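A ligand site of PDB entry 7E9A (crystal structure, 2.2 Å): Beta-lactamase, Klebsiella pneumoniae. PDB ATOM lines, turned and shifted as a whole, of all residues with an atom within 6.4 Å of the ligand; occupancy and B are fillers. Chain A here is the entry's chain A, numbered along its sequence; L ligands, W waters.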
ATOM      1  N   LEU A  43     -31.233   5.684  31.572  1.00  0.00           N
ATOM      2  CA  LEU A  43     -31.811   5.509  30.257  1.00  0.00           C
ATOM      3  C   LEU A  43     -30.822   4.877  29.285  1.00  0.00           C
ATOM      4  O   LEU A  43     -31.205   4.014  28.483  1.00  0.00           O
ATOM      5  CB  LEU A  43     -32.279   6.854  29.731  1.00  0.00           C
ATOM      6  CG  LEU A  43     -33.441   7.535  30.437  1.00  0.00           C
ATOM      7  CD1 LEU A  43     -33.470   9.069  30.183  1.00  0.00           C
ATOM      8  CD2 LEU A  43     -34.751   6.946  30.040  1.00  0.00           C
ATOM      9  N   CYS A  44     -29.568   5.285  29.311  1.00  0.00           N
ATOM     10  CA  CYS A  44     -28.609   4.860  28.304  1.00  0.00           C
ATOM     11  C   CYS A  44     -29.180   5.273  26.956  1.00  0.00           C
ATOM     12  O   CYS A  44     -29.838   6.319  26.839  1.00  0.00           O
ATOM     13  CB  CYS A  44     -28.300   3.342  28.464  1.00  0.00           C
ATOM     14  SG  CYS A  44     -27.899   2.801  30.144  1.00  0.00           S
ATOM     15  N   SER A  45     -29.009   4.471  25.916  1.00  0.00           N
ATOM     16  CA  SER A  45     -29.489   4.842  24.600  1.00  0.00           C
ATOM     17  C   SER A  45     -30.989   4.799  24.458  1.00  0.00           C
ATOM     18  O   SER A  45     -31.494   5.260  23.436  1.00  0.00           O
ATOM     19  CB  SER A  45     -28.906   3.918  23.544  1.00  0.00           C
ATOM     20  OG  SER A  45     -27.530   4.174  23.394  1.00  0.00           O
ATOM     21  N   SER A  46     -31.722   4.259  25.430  1.00  0.00           N
ATOM     22  CA  SER A  46     -33.154   4.188  25.248  1.00  0.00           C
ATOM     23  C   SER A  46     -33.786   5.563  25.114  1.00  0.00           C
ATOM     24  O   SER A  46     -34.894   5.669  24.586  1.00  0.00           O
ATOM     25  CB  SER A  46     -33.821   3.378  26.378  1.00  0.00           C
ATOM     26  OG  SER A  46     -33.889   4.039  27.601  1.00  0.00           O
ATOM     27  N   LYS A  48     -33.034   7.597  22.950  1.00  0.00           N
ATOM     28  CA  LYS A  48     -33.060   7.868  21.518  1.00  0.00           C
ATOM     29  C   LYS A  48     -34.442   7.612  20.925  1.00  0.00           C
ATOM     30  O   LYS A  48     -34.812   8.281  19.963  1.00  0.00           O
ATOM     31  CB  LYS A  48     -31.996   7.039  20.823  1.00  0.00           C
ATOM     32  CG  LYS A  48     -30.607   7.491  21.183  1.00  0.00           C
ATOM     33  CD  LYS A  48     -29.537   6.462  20.904  1.00  0.00           C
ATOM     34  CE  LYS A  48     -28.227   6.886  21.547  1.00  0.00           C
ATOM     35  NZ  LYS A  48     -27.156   5.999  21.200  1.00  0.00           N
ATOM     36  N   PRO A  79     -17.905   7.481  19.202  1.00  0.00           N
ATOM     37  CA  PRO A  79     -17.913   6.016  19.127  1.00  0.00           C
ATOM     38  C   PRO A  79     -19.306   5.444  18.976  1.00  0.00           C
ATOM     39  O   PRO A  79     -20.284   5.959  19.527  1.00  0.00           O
ATOM     40  CB  PRO A  79     -17.293   5.604  20.462  1.00  0.00           C
ATOM     41  CG  PRO A  79     -16.427   6.733  20.826  1.00  0.00           C
ATOM     42  CD  PRO A  79     -17.091   7.962  20.307  1.00  0.00           C
ATOM     43  N   TRP A  80     -19.389   4.332  18.259  1.00  0.00           N
ATOM     44  CA  TRP A  80     -20.629   3.688  17.886  1.00  0.00           C
ATOM     45  C   TRP A  80     -21.593   4.655  17.214  1.00  0.00           C
ATOM     46  O   TRP A  80     -22.622   5.093  17.746  1.00  0.00           O
ATOM     47  CB  TRP A  80     -21.309   3.007  19.069  1.00  0.00           C
ATOM     48  CG  TRP A  80     -22.467   2.203  18.505  1.00  0.00           C
ATOM     49  CD1 TRP A  80     -23.793   2.524  18.553  1.00  0.00           C
ATOM     50  CD2 TRP A  80     -22.379   1.002  17.730  1.00  0.00           C
ATOM     51  NE1 TRP A  80     -24.528   1.591  17.902  1.00  0.00           N
ATOM     52  CE2 TRP A  80     -23.693   0.629  17.390  1.00  0.00           C
ATOM     53  CE3 TRP A  80     -21.313   0.194  17.303  1.00  0.00           C
ATOM     54  CZ2 TRP A  80     -23.983  -0.508  16.635  1.00  0.00           C
ATOM     55  CZ3 TRP A  80     -21.595  -0.948  16.548  1.00  0.00           C
ATOM     56  CH2 TRP A  80     -22.931  -1.281  16.227  1.00  0.00           C
ATOM     57  N   TYR A 104     -30.265   1.798  15.078  1.00  0.00           N
ATOM     58  CA  TYR A 104     -28.893   1.401  15.274  1.00  0.00           C
ATOM     59  C   TYR A 104     -28.314   2.024  16.511  1.00  0.00           C
ATOM     60  O   TYR A 104     -27.164   1.733  16.847  1.00  0.00           O
ATOM     61  CB  TYR A 104     -28.018   1.774  14.041  1.00  0.00           C
ATOM     62  CG  TYR A 104     -28.383   0.951  12.850  1.00  0.00           C
ATOM     63  CD1 TYR A 104     -29.425   1.339  12.024  1.00  0.00           C
ATOM     64  CD2 TYR A 104     -27.766  -0.270  12.596  1.00  0.00           C
ATOM     65  CE1 TYR A 104     -29.815   0.576  10.950  1.00  0.00           C
ATOM     66  CE2 TYR A 104     -28.182  -1.074  11.502  1.00  0.00           C
ATOM     67  CZ  TYR A 104     -29.202  -0.616  10.689  1.00  0.00           C
ATOM     68  OH  TYR A 104     -29.637  -1.323   9.605  1.00  0.00           O
ATOM     69  N   SER A 105     -29.063   2.856  17.206  1.00  0.00           N
ATOM     70  CA  SER A 105     -28.550   3.521  18.384  1.00  0.00           C
ATOM     71  C   SER A 105     -27.383   4.447  18.046  1.00  0.00           C
ATOM     72  O   SER A 105     -26.520   4.695  18.869  1.00  0.00           O
ATOM     73  CB  SER A 105     -28.139   2.486  19.429  1.00  0.00           C
ATOM     74  OG  SER A 105     -28.648   2.863  20.667  1.00  0.00           O
ATOM     75  N   ASN A 107     -24.907   7.136  17.806  1.00  0.00           N
ATOM     76  CA  ASN A 107     -24.663   8.181  18.797  1.00  0.00           C
ATOM     77  C   ASN A 107     -24.514   9.564  18.176  1.00  0.00           C
ATOM     78  O   ASN A 107     -24.975  10.551  18.751  1.00  0.00           O
ATOM     79  CB  ASN A 107     -23.428   7.869  19.638  1.00  0.00           C
ATOM     80  CG  ASN A 107     -23.730   6.900  20.724  1.00  0.00           C
ATOM     81  OD1 ASN A 107     -24.716   7.050  21.442  1.00  0.00           O
ATOM     82  ND2 ASN A 107     -22.865   5.896  20.879  1.00  0.00           N
ATOM     83  N   GLU A 141     -24.203  12.417  24.539  1.00  0.00           N
ATOM     84  CA  GLU A 141     -23.422  11.207  24.288  1.00  0.00           C
ATOM     85  C   GLU A 141     -21.920  11.568  24.236  1.00  0.00           C
ATOM     86  O   GLU A 141     -21.590  12.595  23.687  1.00  0.00           O
ATOM     87  CB  GLU A 141     -23.863  10.551  22.977  1.00  0.00           C
ATOM     88  CG  GLU A 141     -25.268   9.846  23.006  1.00  0.00           C
ATOM     89  CD  GLU A 141     -25.292   8.596  23.873  1.00  0.00           C
ATOM     90  OE1 GLU A 141     -24.241   8.223  24.422  1.00  0.00           O
ATOM     91  OE2 GLU A 141     -26.363   8.003  24.026  1.00  0.00           O
ATOM     92  N   LEU A 142     -21.014  10.799  24.837  1.00  0.00           N
ATOM     93  CA  LEU A 142     -21.260   9.568  25.579  1.00  0.00           C
ATOM     94  C   LEU A 142     -21.352   9.724  27.115  1.00  0.00           C
ATOM     95  O   LEU A 142     -21.474   8.731  27.808  1.00  0.00           O
ATOM     96  CB  LEU A 142     -20.138   8.580  25.278  1.00  0.00           C
ATOM     97  CG  LEU A 142     -20.259   7.670  24.045  1.00  0.00           C
ATOM     98  CD1 LEU A 142     -20.761   8.398  22.887  1.00  0.00           C
ATOM     99  CD2 LEU A 142     -18.869   7.176  23.742  1.00  0.00           C
ATOM    100  N   LEU A 144     -23.655  10.720  29.153  1.00  0.00           N
ATOM    101  CA  LEU A 144     -24.881  10.307  29.821  1.00  0.00           C
ATOM    102  C   LEU A 144     -24.889   8.834  30.213  1.00  0.00           C
ATOM    103  O   LEU A 144     -25.808   8.413  30.909  1.00  0.00           O
ATOM    104  CB  LEU A 144     -26.074  10.624  28.924  1.00  0.00           C
ATOM    105  CG  LEU A 144     -26.167   9.965  27.555  1.00  0.00           C
ATOM    106  CD1 LEU A 144     -26.707   8.543  27.674  1.00  0.00           C
ATOM    107  CD2 LEU A 144     -27.030  10.818  26.669  1.00  0.00           C
ATOM    108  N   ASN A 145     -23.885   8.058  29.791  1.00  0.00           N
ATOM    109  CA  ASN A 145     -23.798   6.631  30.064  1.00  0.00           C
ATOM    110  C   ASN A 145     -23.077   6.295  31.363  1.00  0.00           C
ATOM    111  O   ASN A 145     -22.900   5.113  31.644  1.00  0.00           O
ATOM    112  CB  ASN A 145     -23.085   5.933  28.911  1.00  0.00           C
ATOM    113  CG  ASN A 145     -23.871   6.024  27.605  1.00  0.00           C
ATOM    114  OD1 ASN A 145     -25.031   5.629  27.530  1.00  0.00           O
ATOM    115  ND2 ASN A 145     -23.256   6.582  26.581  1.00  0.00           N
ATOM    116  N   THR A 191     -31.171  -3.843  17.133  1.00  0.00           N
ATOM    117  CA  THR A 191     -30.277  -4.018  18.267  1.00  0.00           C
ATOM    118  C   THR A 191     -30.848  -4.866  19.379  1.00  0.00           C
ATOM    119  O   THR A 191     -30.136  -5.125  20.357  1.00  0.00           O
ATOM    120  CB  THR A 191     -29.892  -2.658  18.862  1.00  0.00           C
ATOM    121  OG1 THR A 191     -31.073  -1.986  19.299  1.00  0.00           O
ATOM    122  CG2 THR A 191     -29.179  -1.809  17.831  1.00  0.00           C
ATOM    123  N   ARG A 195     -33.260  -9.383  23.662  1.00  0.00           N
ATOM    124  CA  ARG A 195     -33.878  -8.723  24.810  1.00  0.00           C
ATOM    125  C   ARG A 195     -35.375  -9.013  24.726  1.00  0.00           C
ATOM    126  O   ARG A 195     -35.752 -10.180  24.720  1.00  0.00           O
ATOM    127  CB  ARG A 195     -33.483  -7.253  24.871  1.00  0.00           C
ATOM    128  CG  ARG A 195     -31.986  -7.157  25.040  1.00  0.00           C
ATOM    129  CD  ARG A 195     -31.486  -5.786  25.346  1.00  0.00           C
ATOM    130  NE  ARG A 195     -30.028  -5.777  25.368  1.00  0.00           N
ATOM    131  CZ  ARG A 195     -29.281  -4.739  25.690  1.00  0.00           C
ATOM    132  NH1 ARG A 195     -29.801  -3.564  26.046  1.00  0.00           N
ATOM    133  NH2 ARG A 195     -27.986  -4.868  25.678  1.00  0.00           N
ATOM    134  N   LYS A 209     -36.695  -0.387  21.556  1.00  0.00           N
ATOM    135  CA  LYS A 209     -35.497   0.432  21.653  1.00  0.00           C
ATOM    136  C   LYS A 209     -34.688  -0.049  22.845  1.00  0.00           C
ATOM    137  O   LYS A 209     -35.201  -0.121  23.962  1.00  0.00           O
ATOM    138  CB  LYS A 209     -35.851   1.917  21.791  1.00  0.00           C
ATOM    139  CG  LYS A 209     -34.627   2.847  21.920  1.00  0.00           C
ATOM    140  CD  LYS A 209     -33.741   2.789  20.730  1.00  0.00           C
ATOM    141  CE  LYS A 209     -32.382   3.369  20.980  1.00  0.00           C
ATOM    142  NZ  LYS A 209     -31.271   2.392  20.834  1.00  0.00           N
ATOM    143  N   THR A 210     -33.430  -0.413  22.599  1.00  0.00           N
ATOM    144  CA  THR A 210     -32.491  -0.890  23.602  1.00  0.00           C
ATOM    145  C   THR A 210     -31.646   0.223  24.192  1.00  0.00           C
ATOM    146  O   THR A 210     -31.492   1.307  23.617  1.00  0.00           O
ATOM    147  CB  THR A 210     -31.530  -1.904  23.009  1.00  0.00           C
ATOM    148  OG1 THR A 210     -30.852  -1.330  21.894  1.00  0.00           O
ATOM    149  CG2 THR A 210     -32.240  -3.113  22.544  1.00  0.00           C
ATOM    150  N   GLY A 211     -31.021  -0.069  25.318  1.00  0.00           N
ATOM    151  CA  GLY A 211     -29.974   0.765  25.872  1.00  0.00           C
ATOM    152  C   GLY A 211     -28.940  -0.018  26.632  1.00  0.00           C
ATOM    153  O   GLY A 211     -29.273  -1.007  27.279  1.00  0.00           O
ATOM    154  N   THR A 212     -27.662   0.363  26.497  1.00  0.00           N
ATOM    155  CA  THR A 212     -26.569  -0.281  27.204  1.00  0.00           C
ATOM    156  C   THR A 212     -25.547   0.779  27.601  1.00  0.00           C
ATOM    157  O   THR A 212     -24.920   1.399  26.731  1.00  0.00           O
ATOM    158  CB  THR A 212     -25.895  -1.380  26.367  1.00  0.00           C
ATOM    159  OG1 THR A 212     -26.875  -2.259  25.830  1.00  0.00           O
ATOM    160  CG2 THR A 212     -24.893  -2.225  27.214  1.00  0.00           C
ATOM    161  N   CYS A 213     -25.377   0.970  28.908  1.00  0.00           N
ATOM    162  CA  CYS A 213     -24.478   1.995  29.403  1.00  0.00           C
ATOM    163  C   CYS A 213     -23.047   1.529  29.411  1.00  0.00           C
ATOM    164  O   CYS A 213     -22.142   2.361  29.297  1.00  0.00           O
ATOM    165  CB  CYS A 213     -24.887   2.461  30.796  1.00  0.00           C
ATOM    166  SG  CYS A 213     -26.193   3.786  30.813  1.00  0.00           S
ATOM    167  N   ALA A 219     -28.402  -1.872  31.576  1.00  0.00           N
ATOM    168  CA  ALA A 219     -28.939  -2.041  30.219  1.00  0.00           C
ATOM    169  C   ALA A 219     -30.452  -2.165  30.285  1.00  0.00           C
ATOM    170  O   ALA A 219     -31.026  -2.460  31.330  1.00  0.00           O
ATOM    171  CB  ALA A 219     -28.353  -3.248  29.511  1.00  0.00           C
ATOM    172  N   ASN A 220     -31.084  -1.995  29.127  1.00  0.00           N
ATOM    173  CA  ASN A 220     -32.537  -1.906  29.117  1.00  0.00           C
ATOM    174  C   ASN A 220     -33.096  -2.112  27.718  1.00  0.00           C
ATOM    175  O   ASN A 220     -32.380  -2.214  26.731  1.00  0.00           O
ATOM    176  CB  ASN A 220     -32.952  -0.559  29.682  1.00  0.00           C
ATOM    177  CG  ASN A 220     -32.250   0.566  28.988  1.00  0.00           C
ATOM    178  OD1 ASN A 220     -32.436   0.736  27.790  1.00  0.00           O
ATOM    179  ND2 ASN A 220     -31.416   1.308  29.710  1.00  0.00           N
ATOM    180  N   GLU A 250     -28.195  -9.647  28.781  1.00  0.00           N
ATOM    181  CA  GLU A 250     -29.354  -9.641  27.881  1.00  0.00           C
ATOM    182  C   GLU A 250     -30.374 -10.722  28.262  1.00  0.00           C
ATOM    183  O   GLU A 250     -31.584 -10.507  28.167  1.00  0.00           O
ATOM    184  CB  GLU A 250     -28.864  -9.822  26.453  1.00  0.00           C
ATOM    185  CG  GLU A 250     -28.045  -8.634  25.972  1.00  0.00           C
ATOM    186  CD  GLU A 250     -28.007  -8.543  24.462  1.00  0.00           C
ATOM    187  OE1 GLU A 250     -27.368  -9.427  23.859  1.00  0.00           O
ATOM    188  OE2 GLU A 250     -28.649  -7.627  23.890  1.00  0.00           O
HETATM  189  C1  LIG L   1     -22.669   3.653  23.175  1.00  0.00           C
HETATM  190  C2  LIG L   1     -22.475   2.625  22.305  1.00  0.00           C
HETATM  191  C3  LIG L   1     -23.504   1.774  21.957  1.00  0.00           C
HETATM  192  C4  LIG L   1     -24.790   1.933  22.514  1.00  0.00           C
HETATM  193  C5  LIG L   1     -24.972   2.960  23.348  1.00  0.00           C
HETATM  194  C6  LIG L   1     -23.919   3.829  23.710  1.00  0.00           C
HETATM  195  B1  LIG L   1     -26.422   2.904  23.852  1.00  0.00           B
HETATM  196  O1  LIG L   1     -27.080   1.901  23.092  1.00  0.00           O
HETATM  197  C7  LIG L   1     -26.116   1.188  22.306  1.00  0.00           C
HETATM  198  C8  LIG L   1     -26.218  -0.249  22.660  1.00  0.00           C
HETATM  199  C9  LIG L   1     -25.187  -1.012  22.945  1.00  0.00           C
HETATM  200  C10 LIG L   1     -27.634  -0.845  22.672  1.00  0.00           C
HETATM  201  O2  LIG L   1     -27.998  -1.648  23.560  1.00  0.00           O
HETATM  202  O3  LIG L   1     -28.431  -0.528  21.761  1.00  0.00           O
HETATM  203  O4  LIG L   1     -26.944   2.883  25.116  1.00  0.00           O
HETATM  204  O   HOH W   1     -28.570  -4.036  22.619  1.00  0.00           O
HETATM  205  O   HOH W   2     -26.408   5.952  25.363  1.00  0.00           O
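An oxygen (O4) of the ligand lies close to the backbone NH of Ser 45, at 2.7 Å.
A boron (B1) of the ligand is bonded to the side-chain hydroxyl of Ser 45, 1.7 Å away.
The side-chain hydroxyl (OG1) of Thr 210 lies within hydrogen-bond range of an oxygen (O3) of the ligand.
An oxygen (O4) of the ligand sits at hydrogen-bond distance from the backbone NH (N) of Thr 212.
O of Thr 212 sits at hydrogen-bond distance from O4 of the ligand.
The side-chain hydroxyl of Thr 212 lies within hydrogen-bond range of an oxygen (O2) of the ligand, at 2.6 Å.
The side-chain hydroxyl (OG) of Ser 105 sits at hydrogen-bond distance from an oxygen (O1) of the ligand, 3.0 Å away.
The guanidinium group (NH1) of Arg 195 is in salt-bridge range of an oxygen (O2) of the ligand, at 3.6 Å.
The side-chain hydroxyl (OG) of Ser 45 sits close to the side-chain hydroxyl (OG) of Ser 105 (3.2 Å).
The side-chain hydroxyl (OG1) of Thr 210 is in hydrogen-bond range of the side-chain hydroxyl (OG1) of Thr 191.
The side-chain hydroxyl (OG1) of Thr 212 lies within hydrogen-bond range of the guanidinium group (NH2) of Arg 195 (2.8 Å).
N of Asn 107 is in hydrogen-bond range of O of Trp 80 (3.1 Å).
The side-chain amide nitrogen (ND2) of Asn 107 lies within hydrogen-bond range of the backbone carbonyl oxygen (O) of Pro 79, at 2.9 Å.
The indole nitrogen (NE1) of Trp 80 is in hydrogen-bond range of the backbone carbonyl oxygen (O) of Tyr 104.
The side-chain carboxylate of Glu 250 lies within salt-bridge range of the guanidinium group of Arg 195 (2.7 Å).
SG of Cys 44 forms a disulfide with SG of Cys 213 (2.1 Å).
CB of Cys 44 touches O4 of the ligand, 3.6 Å away.
Trp 80 touches the ligand (CB to C2, 3.5 Å).
Asn 107 touches the ligand (ND2 to C1, 3.2 Å).
Thr 191 touches the ligand.
Gly 211 touches the ligand.
Hydrophobic or aromatic side chains that line the ligand: Trp 80.
Water W1 lies within hydrogen-bond range of an oxygen (O2) of the ligand, the backbone carbonyl oxygen (O) of Thr 191 and the guanidinium group (NH2) of Arg 195.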
